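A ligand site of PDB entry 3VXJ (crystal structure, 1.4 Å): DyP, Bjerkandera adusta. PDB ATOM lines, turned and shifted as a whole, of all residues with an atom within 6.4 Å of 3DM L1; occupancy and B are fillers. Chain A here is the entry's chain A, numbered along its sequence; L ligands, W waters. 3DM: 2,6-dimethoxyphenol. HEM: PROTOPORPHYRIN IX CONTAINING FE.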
ATOM      1  N   SER A 174      23.640  14.476  -6.006  1.00  0.00           N
ATOM      2  CA  SER A 174      24.666  13.466  -5.760  1.00  0.00           C
ATOM      3  C   SER A 174      26.015  14.063  -5.348  1.00  0.00           C
ATOM      4  O   SER A 174      26.667  14.749  -6.136  1.00  0.00           O
ATOM      5  CB  SER A 174      24.846  12.565  -6.988  1.00  0.00           C
ATOM      6  OG  SER A 174      25.748  11.533  -6.675  1.00  0.00           O
ATOM      7  N   GLY A 188      23.222   4.580  -2.056  1.00  0.00           N
ATOM      8  CA  GLY A 188      23.854   4.875  -3.338  1.00  0.00           C
ATOM      9  C   GLY A 188      24.936   5.938  -3.274  1.00  0.00           C
ATOM     10  O   GLY A 188      25.685   6.125  -4.222  1.00  0.00           O
ATOM     11  N   GLN A 189      25.011   6.639  -2.149  1.00  0.00           N
ATOM     12  CA  GLN A 189      26.013   7.674  -1.961  1.00  0.00           C
ATOM     13  C   GLN A 189      27.391   7.030  -1.765  1.00  0.00           C
ATOM     14  O   GLN A 189      27.536   6.058  -1.013  1.00  0.00           O
ATOM     15  CB  GLN A 189      25.619   8.535  -0.763  1.00  0.00           C
ATOM     16  CG  GLN A 189      26.485   9.732  -0.582  1.00  0.00           C
ATOM     17  CD  GLN A 189      25.948  10.746   0.410  1.00  0.00           C
ATOM     18  OE1 GLN A 189      25.171  10.432   1.315  1.00  0.00           O
ATOM     19  NE2 GLN A 189      26.375  11.985   0.249  1.00  0.00           N
ATOM     20  N   ALA A 190      28.400   7.554  -2.473  1.00  0.00           N
ATOM     21  CA  ALA A 190      29.764   7.057  -2.317  1.00  0.00           C
ATOM     22  C   ALA A 190      30.340   7.538  -0.996  1.00  0.00           C
ATOM     23  O   ALA A 190      30.196   8.712  -0.631  1.00  0.00           O
ATOM     24  CB  ALA A 190      30.646   7.518  -3.472  1.00  0.00           C
ATOM     25  N   ASN A 289      19.426   8.497  -5.430  1.00  0.00           N
ATOM     26  CA  ASN A 289      20.816   8.204  -5.748  1.00  0.00           C
ATOM     27  C   ASN A 289      21.143   6.710  -5.684  1.00  0.00           C
ATOM     28  O   ASN A 289      22.297   6.309  -5.843  1.00  0.00           O
ATOM     29  CB  ASN A 289      21.766   8.987  -4.839  1.00  0.00           C
ATOM     30  CG  ASN A 289      22.926   9.577  -5.621  1.00  0.00           C
ATOM     31  OD1 ASN A 289      22.875   9.679  -6.846  1.00  0.00           O
ATOM     32  ND2 ASN A 289      23.960  10.001  -4.906  1.00  0.00           N
ATOM     33  N   ASN A 290      20.121   5.883  -5.486  1.00  0.00           N
ATOM     34  CA  ASN A 290      20.314   4.454  -5.271  1.00  0.00           C
ATOM     35  C   ASN A 290      20.311   3.634  -6.559  1.00  0.00           C
ATOM     36  O   ASN A 290      19.425   2.821  -6.807  1.00  0.00           O
ATOM     37  CB  ASN A 290      19.281   3.932  -4.284  1.00  0.00           C
ATOM     38  CG  ASN A 290      19.687   2.610  -3.677  1.00  0.00           C
ATOM     39  OD1 ASN A 290      20.828   2.181  -3.819  1.00  0.00           O
ATOM     40  ND2 ASN A 290      18.751   1.944  -3.016  1.00  0.00           N
ATOM     41  N   PHE A 291      21.339   3.853  -7.372  1.00  0.00           N
ATOM     42  CA  PHE A 291      21.504   3.183  -8.659  1.00  0.00           C
ATOM     43  C   PHE A 291      22.986   3.223  -8.987  1.00  0.00           C
ATOM     44  O   PHE A 291      23.722   4.080  -8.454  1.00  0.00           O
ATOM     45  CB  PHE A 291      20.706   3.890  -9.767  1.00  0.00           C
ATOM     46  CG  PHE A 291      21.161   5.290 -10.059  1.00  0.00           C
ATOM     47  CD1 PHE A 291      22.091   5.549 -11.080  1.00  0.00           C
ATOM     48  CD2 PHE A 291      20.709   6.357  -9.291  1.00  0.00           C
ATOM     49  CE1 PHE A 291      22.528   6.848 -11.338  1.00  0.00           C
ATOM     50  CE2 PHE A 291      21.155   7.661  -9.546  1.00  0.00           C
ATOM     51  CZ  PHE A 291      22.061   7.901 -10.567  1.00  0.00           C
ATOM     52  N   ASP A 292      23.435   2.334  -9.849  1.00  0.00           N
ATOM     53  CA  ASP A 292      24.861   2.277 -10.175  1.00  0.00           C
ATOM     54  C   ASP A 292      25.164   1.887 -11.623  1.00  0.00           C
ATOM     55  O   ASP A 292      26.321   1.624 -11.943  1.00  0.00           O
ATOM     56  CB  ASP A 292      25.608   1.355  -9.201  1.00  0.00           C
ATOM     57  CG  ASP A 292      25.121  -0.092  -9.235  1.00  0.00           C
ATOM     58  OD1 ASP A 292      24.267  -0.426 -10.088  1.00  0.00           O
ATOM     59  OD2 ASP A 292      25.603  -0.899  -8.414  1.00  0.00           O
ATOM     60  N   ASN A 313      30.209  10.760 -13.187  1.00  0.00           N
ATOM     61  CA  ASN A 313      30.351   9.696 -12.191  1.00  0.00           C
ATOM     62  C   ASN A 313      29.909   8.370 -12.778  1.00  0.00           C
ATOM     63  O   ASN A 313      28.714   8.036 -12.740  1.00  0.00           O
ATOM     64  CB  ASN A 313      29.568  10.012 -10.911  1.00  0.00           C
ATOM     65  CG  ASN A 313      29.675   8.886  -9.884  1.00  0.00           C
ATOM     66  OD1 ASN A 313      30.467   7.939 -10.050  1.00  0.00           O
ATOM     67  ND2 ASN A 313      28.864   8.975  -8.836  1.00  0.00           N
ATOM     68  N   PRO A 314      30.862   7.602 -13.324  1.00  0.00           N
ATOM     69  CA  PRO A 314      30.537   6.376 -14.044  1.00  0.00           C
ATOM     70  C   PRO A 314      30.023   5.227 -13.184  1.00  0.00           C
ATOM     71  O   PRO A 314      29.538   4.251 -13.743  1.00  0.00           O
ATOM     72  CB  PRO A 314      31.863   5.995 -14.706  1.00  0.00           C
ATOM     73  CG  PRO A 314      32.643   7.275 -14.763  1.00  0.00           C
ATOM     74  CD  PRO A 314      32.267   7.999 -13.515  1.00  0.00           C
ATOM     75  N   ARG A 315      30.107   5.320 -11.853  1.00  0.00           N
ATOM     76  CA  ARG A 315      29.611   4.260 -10.968  1.00  0.00           C
ATOM     77  C   ARG A 315      30.127   2.892 -11.449  1.00  0.00           C
ATOM     78  O   ARG A 315      31.347   2.741 -11.621  1.00  0.00           O
ATOM     79  CB  ARG A 315      28.074   4.349 -10.788  1.00  0.00           C
ATOM     80  CG  ARG A 315      27.646   5.713 -10.285  1.00  0.00           C
ATOM     81  CD  ARG A 315      26.156   5.810  -9.967  1.00  0.00           C
ATOM     82  NE  ARG A 315      25.832   7.214  -9.690  1.00  0.00           N
ATOM     83  CZ  ARG A 315      25.010   7.666  -8.744  1.00  0.00           C
ATOM     84  NH1 ARG A 315      24.376   6.834  -7.929  1.00  0.00           N
ATOM     85  NH2 ARG A 315      24.848   8.964  -8.605  1.00  0.00           N
ATOM     86  N   GLN A 316      29.250   1.898 -11.660  1.00  0.00           N
ATOM     87  CA  GLN A 316      29.704   0.551 -12.002  1.00  0.00           C
ATOM     88  C   GLN A 316      30.323   0.424 -13.396  1.00  0.00           C
ATOM     89  O   GLN A 316      30.923  -0.610 -13.705  1.00  0.00           O
ATOM     90  CB  GLN A 316      28.564  -0.474 -11.815  1.00  0.00           C
ATOM     91  CG  GLN A 316      28.982  -1.959 -11.880  1.00  0.00           C
ATOM     92  CD  GLN A 316      29.899  -2.388 -10.741  1.00  0.00           C
ATOM     93  OE1 GLN A 316      29.909  -1.778  -9.675  1.00  0.00           O
ATOM     94  NE2 GLN A 316      30.643  -3.457 -10.970  1.00  0.00           N
ATOM     95  N   LEU A 318      32.958   1.682 -14.007  1.00  0.00           N
ATOM     96  CA  LEU A 318      34.367   1.528 -13.638  1.00  0.00           C
ATOM     97  C   LEU A 318      34.714   0.125 -13.125  1.00  0.00           C
ATOM     98  O   LEU A 318      35.896  -0.192 -12.964  1.00  0.00           O
ATOM     99  CB  LEU A 318      34.776   2.584 -12.597  1.00  0.00           C
ATOM    100  CG  LEU A 318      34.715   4.042 -13.038  1.00  0.00           C
ATOM    101  CD1 LEU A 318      35.193   4.932 -11.913  1.00  0.00           C
ATOM    102  CD2 LEU A 318      35.530   4.283 -14.303  1.00  0.00           C
ATOM    103  N   GLY A 320      33.451  -1.207 -10.217  1.00  0.00           N
ATOM    104  CA  GLY A 320      33.214  -1.249  -8.780  1.00  0.00           C
ATOM    105  C   GLY A 320      33.457   0.125  -8.185  1.00  0.00           C
ATOM    106  O   GLY A 320      33.734   1.077  -8.928  1.00  0.00           O
ATOM    107  N   PRO A 321      33.326   0.252  -6.843  1.00  0.00           N
ATOM    108  CA  PRO A 321      33.594   1.526  -6.166  1.00  0.00           C
ATOM    109  C   PRO A 321      35.042   1.966  -6.380  1.00  0.00           C
ATOM    110  O   PRO A 321      35.959   1.148  -6.322  1.00  0.00           O
ATOM    111  CB  PRO A 321      33.323   1.205  -4.693  1.00  0.00           C
ATOM    112  CG  PRO A 321      32.434   0.008  -4.719  1.00  0.00           C
ATOM    113  CD  PRO A 321      32.871  -0.785  -5.903  1.00  0.00           C
ATOM    114  N   VAL A 322      35.208   3.252  -6.674  1.00  0.00           N
ATOM    115  CA  VAL A 322      36.522   3.850  -6.857  1.00  0.00           C
ATOM    116  C   VAL A 322      36.467   5.181  -6.116  1.00  0.00           C
ATOM    117  O   VAL A 322      35.580   5.989  -6.379  1.00  0.00           O
ATOM    118  CB  VAL A 322      36.841   4.081  -8.380  1.00  0.00           C
ATOM    119  CG1 VAL A 322      38.164   4.831  -8.575  1.00  0.00           C
ATOM    120  CG2 VAL A 322      36.833   2.763  -9.166  1.00  0.00           C
ATOM    121  N   ASP A 323      37.389   5.397  -5.178  1.00  0.00           N
ATOM    122  CA  ASP A 323      37.405   6.617  -4.372  1.00  0.00           C
ATOM    123  C   ASP A 323      37.843   7.836  -5.169  1.00  0.00           C
ATOM    124  O   ASP A 323      37.393   8.945  -4.911  1.00  0.00           O
ATOM    125  CB  ASP A 323      38.409   6.505  -3.201  1.00  0.00           C
ATOM    126  CG  ASP A 323      38.048   5.432  -2.201  1.00  0.00           C
ATOM    127  OD1 ASP A 323      36.862   5.061  -2.089  1.00  0.00           O
ATOM    128  OD2 ASP A 323      38.978   4.992  -1.484  1.00  0.00           O
ATOM    129  N   PHE A 325      37.976   9.620  -8.011  1.00  0.00           N
ATOM    130  CA  PHE A 325      37.464  10.641  -8.932  1.00  0.00           C
ATOM    131  C   PHE A 325      36.195  11.331  -8.475  1.00  0.00           C
ATOM    132  O   PHE A 325      35.561  12.030  -9.261  1.00  0.00           O
ATOM    133  CB  PHE A 325      37.323  10.059 -10.347  1.00  0.00           C
ATOM    134  CG  PHE A 325      38.497   9.234 -10.764  1.00  0.00           C
ATOM    135  CD1 PHE A 325      39.738   9.824 -10.997  1.00  0.00           C
ATOM    136  CD2 PHE A 325      38.365   7.845 -10.884  1.00  0.00           C
ATOM    137  CE1 PHE A 325      40.843   9.040 -11.364  1.00  0.00           C
ATOM    138  CE2 PHE A 325      39.470   7.061 -11.251  1.00  0.00           C
ATOM    139  CZ  PHE A 325      40.709   7.659 -11.491  1.00  0.00           C
ATOM    140  N   HIS A 326      35.851  11.155  -7.198  1.00  0.00           N
ATOM    141  CA  HIS A 326      34.714  11.854  -6.616  1.00  0.00           C
ATOM    142  C   HIS A 326      35.107  13.276  -6.220  1.00  0.00           C
ATOM    143  O   HIS A 326      36.251  13.536  -5.880  1.00  0.00           O
ATOM    144  CB  HIS A 326      34.154  11.076  -5.435  1.00  0.00           C
ATOM    145  CG  HIS A 326      33.570   9.753  -5.818  1.00  0.00           C
ATOM    146  ND1 HIS A 326      32.373   9.632  -6.488  1.00  0.00           N
ATOM    147  CD2 HIS A 326      34.034   8.487  -5.662  1.00  0.00           C
ATOM    148  CE1 HIS A 326      32.113   8.356  -6.717  1.00  0.00           C
ATOM    149  NE2 HIS A 326      33.119   7.644  -6.235  1.00  0.00           N
ATOM    150  N   TRP A 374      36.876  11.824 -19.230  1.00  0.00           N
ATOM    151  CA  TRP A 374      35.550  11.240 -19.305  1.00  0.00           C
ATOM    152  C   TRP A 374      34.616  11.980 -20.280  1.00  0.00           C
ATOM    153  O   TRP A 374      34.313  11.450 -21.347  1.00  0.00           O
ATOM    154  CB  TRP A 374      34.947  11.101 -17.913  1.00  0.00           C
ATOM    155  CG  TRP A 374      35.647  10.052 -17.075  1.00  0.00           C
ATOM    156  CD1 TRP A 374      36.542   9.101 -17.506  1.00  0.00           C
ATOM    157  CD2 TRP A 374      35.490   9.842 -15.669  1.00  0.00           C
ATOM    158  NE1 TRP A 374      36.936   8.309 -16.452  1.00  0.00           N
ATOM    159  CE2 TRP A 374      36.315   8.753 -15.313  1.00  0.00           C
ATOM    160  CE3 TRP A 374      34.744  10.483 -14.671  1.00  0.00           C
ATOM    161  CZ2 TRP A 374      36.395   8.270 -14.019  1.00  0.00           C
ATOM    162  CZ3 TRP A 374      34.832  10.010 -13.382  1.00  0.00           C
ATOM    163  CH2 TRP A 374      35.647   8.915 -13.058  1.00  0.00           C
HETATM  164  O1  3DM L   1      29.449   6.524  -6.971  1.00  0.00           O
HETATM  165  C1  3DM L   1      29.636   5.182  -7.237  1.00  0.00           C
HETATM  166  C2  3DM L   1      30.844   4.708  -7.773  1.00  0.00           C
HETATM  167  O2  3DM L   1      31.848   5.615  -8.046  1.00  0.00           O
HETATM  168  C7  3DM L   1      32.900   5.197  -8.929  1.00  0.00           C
HETATM  169  C3  3DM L   1      30.991   3.340  -8.015  1.00  0.00           C
HETATM  170  C4  3DM L   1      29.943   2.459  -7.753  1.00  0.00           C
HETATM  171  C5  3DM L   1      28.749   2.924  -7.214  1.00  0.00           C
HETATM  172  C6  3DM L   1      28.604   4.285  -6.964  1.00  0.00           C
HETATM  173  O3  3DM L   1      27.452   4.809  -6.432  1.00  0.00           O
HETATM  174  C8  3DM L   1      26.273   3.955  -6.438  1.00  0.00           C
HETATM  175  CHA HEM L   2      25.491  16.272 -11.715  1.00  0.00           C
HETATM  176  CHB HEM L   2      24.036  20.108 -14.286  1.00  0.00           C
HETATM  177  CHC HEM L   2      28.628  21.164 -15.373  1.00  0.00           C
HETATM  178  CHD HEM L   2      30.108  17.357 -12.780  1.00  0.00           C
HETATM  179  C1A HEM L   2      24.701  17.192 -12.342  1.00  0.00           C
HETATM  180  C2A HEM L   2      23.249  17.196 -12.349  1.00  0.00           C
HETATM  181  C3A HEM L   2      22.851  18.263 -13.068  1.00  0.00           C
HETATM  182  C4A HEM L   2      24.030  18.965 -13.517  1.00  0.00           C
HETATM  183  CMA HEM L   2      21.405  18.703 -13.359  1.00  0.00           C
HETATM  184  CAA HEM L   2      22.364  16.117 -11.679  1.00  0.00           C
HETATM  185  CBA HEM L   2      22.010  16.366 -10.215  1.00  0.00           C
HETATM  186  CGA HEM L   2      23.171  16.156  -9.256  1.00  0.00           C
HETATM  187  O1A HEM L   2      23.603  15.006  -9.030  1.00  0.00           O
HETATM  188  O2A HEM L   2      23.647  17.168  -8.690  1.00  0.00           O
HETATM  189  C1B HEM L   2      25.153  20.738 -14.791  1.00  0.00           C
HETATM  190  C2B HEM L   2      25.144  21.941 -15.613  1.00  0.00           C
HETATM  191  C3B HEM L   2      26.424  22.232 -15.908  1.00  0.00           C
HETATM  192  C4B HEM L   2      27.259  21.240 -15.274  1.00  0.00           C
HETATM  193  CMB HEM L   2      23.864  22.668 -16.050  1.00  0.00           C
HETATM  194  CAB HEM L   2      26.967  23.420 -16.737  1.00  0.00           C
HETATM  195  CBB HEM L   2      26.280  24.550 -16.886  1.00  0.00           C
HETATM  196  C1C HEM L   2      29.420  20.202 -14.800  1.00  0.00           C
HETATM  197  C2C HEM L   2      30.858  20.085 -14.949  1.00  0.00           C
HETATM  198  C3C HEM L   2      31.272  19.017 -14.247  1.00  0.00           C
HETATM  199  C4C HEM L   2      30.098  18.440 -13.630  1.00  0.00           C
HETATM  200  CMC HEM L   2      31.718  21.055 -15.785  1.00  0.00           C
HETATM  201  CAC HEM L   2      32.704  18.460 -14.061  1.00  0.00           C
HETATM  202  CBC HEM L   2      33.601  18.471 -15.060  1.00  0.00           C
HETATM  203  C1D HEM L   2      29.008  16.772 -12.209  1.00  0.00           C
HETATM  204  C2D HEM L   2      29.081  15.704 -11.247  1.00  0.00           C
HETATM  205  C3D HEM L   2      27.659  15.363 -10.933  1.00  0.00           C
HETATM  206  C4D HEM L   2      26.859  16.258 -11.717  1.00  0.00           C
HETATM  207  CMD HEM L   2      30.317  15.016 -10.644  1.00  0.00           C
HETATM  208  CAD HEM L   2      27.229  14.255  -9.953  1.00  0.00           C
HETATM  209  CBD HEM L   2      27.286  12.931 -10.715  1.00  0.00           C
HETATM  210  CGD HEM L   2      26.924  11.769  -9.837  1.00  0.00           C
HETATM  211  O1D HEM L   2      26.043  10.977 -10.258  1.00  0.00           O
HETATM  212  O2D HEM L   2      27.504  11.625  -8.736  1.00  0.00           O
HETATM  213  NA  HEM L   2      25.136  18.266 -13.081  1.00  0.00           N
HETATM  214  NB  HEM L   2      26.468  20.312 -14.630  1.00  0.00           N
HETATM  215  NC  HEM L   2      28.993  19.159 -14.021  1.00  0.00           N
HETATM  216  ND  HEM L   2      27.671  17.103 -12.454  1.00  0.00           N
HETATM  217 FE   HEM L   2      27.061  18.671 -13.609  1.00  0.00          FE
HETATM  218  O   HOH W   1      27.746   7.608  -5.341  1.00  0.00           O
HETATM  219  O   HOH W   2      33.341   8.550  -9.831  1.00  0.00           O
HETATM  220  O   HOH W   3      33.026   4.918  -5.334  1.00  0.00           O
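Water W1 lies within hydrogen-bond range of an oxygen (O1) of 3DM L1 (2.6 Å), the backbone carbonyl oxygen of Gly 188 (2.8 Å) and the backbone NH of Ala 190 (2.9 Å). Water W3 lies within hydrogen-bond range of NE2 of His 326 (2.9 Å), O of Val 322 (3.0 Å) and O2 of 3DM L1 (3.0 Å).
O of Gly 188 lies close to O3 of 3DM L1 (3.1 Å). Ala 190 touches 3DM L1 (CB to O1, 3.8 Å). O of Phe 291 touches C8 of 3DM L1, 3.3 Å away. Asp 292 touches 3DM L1. Arg 315 touches 3DM L1. Leu 318 touches 3DM L1 (CD1 to C7, 3.8 Å). O of Gly 320 touches C3 of 3DM L1, 3.7 Å away. CA of Pro 321 touches C3 of 3DM L1 (3.7 Å). Val 322 touches 3DM L1. Hydrophobic or aromatic side chains within 4 Å of 3DM L1: Ala 190, Leu 318 and His 326. Of the 20 residues printed, 11 come within 4 Å of 3DM L1. Along chain A the residues within 4 Å of 3DM L1 span positions 188 to 326.
NE2 of His 326 sits at hydrogen-bond distance from O of Val 322, at 3.0 Å. The side-chain amide oxygen of Asn 313 lies close to the backbone NH of Arg 315 (3.2 Å). The backbone carbonyl oxygen (O) of Phe 291 lies within hydrogen-bond range of the guanidinium group (NH1) of Arg 315, at 2.9 Å. OD1 of Asn 289 is in hydrogen-bond range of NH2 of Arg 315, 2.7 Å away. NH2 of Arg 315 lies within hydrogen-bond range of OG of Ser 174, 3.3 Å away. The backbone carbonyl oxygen (O) of Asp 292 is in hydrogen-bond range of the backbone NH (N) of Gln 316, at 3.0 Å.
NE2 of His 326 sits at hydrogen-bond distance from O2 of 3DM L1. ND2 of Asn 313 is in hydrogen-bond range of O1 of 3DM L1 (3.1 Å). ND2 of Asn 313 is in hydrogen-bond range of O2D of HEM L2 (3.0 Å). An oxygen (O1D) of HEM L2 lies within salt-bridge range of the guanidinium group (NH2) of Arg 315, 2.9 Å away. The backbone NH (N) of Ser 174 sits at hydrogen-bond distance from an oxygen (O1A) of HEM L2, 3.1 Å away. O2D of HEM L2 lies within hydrogen-bond range of OG of Ser 174, 2.7 Å away.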
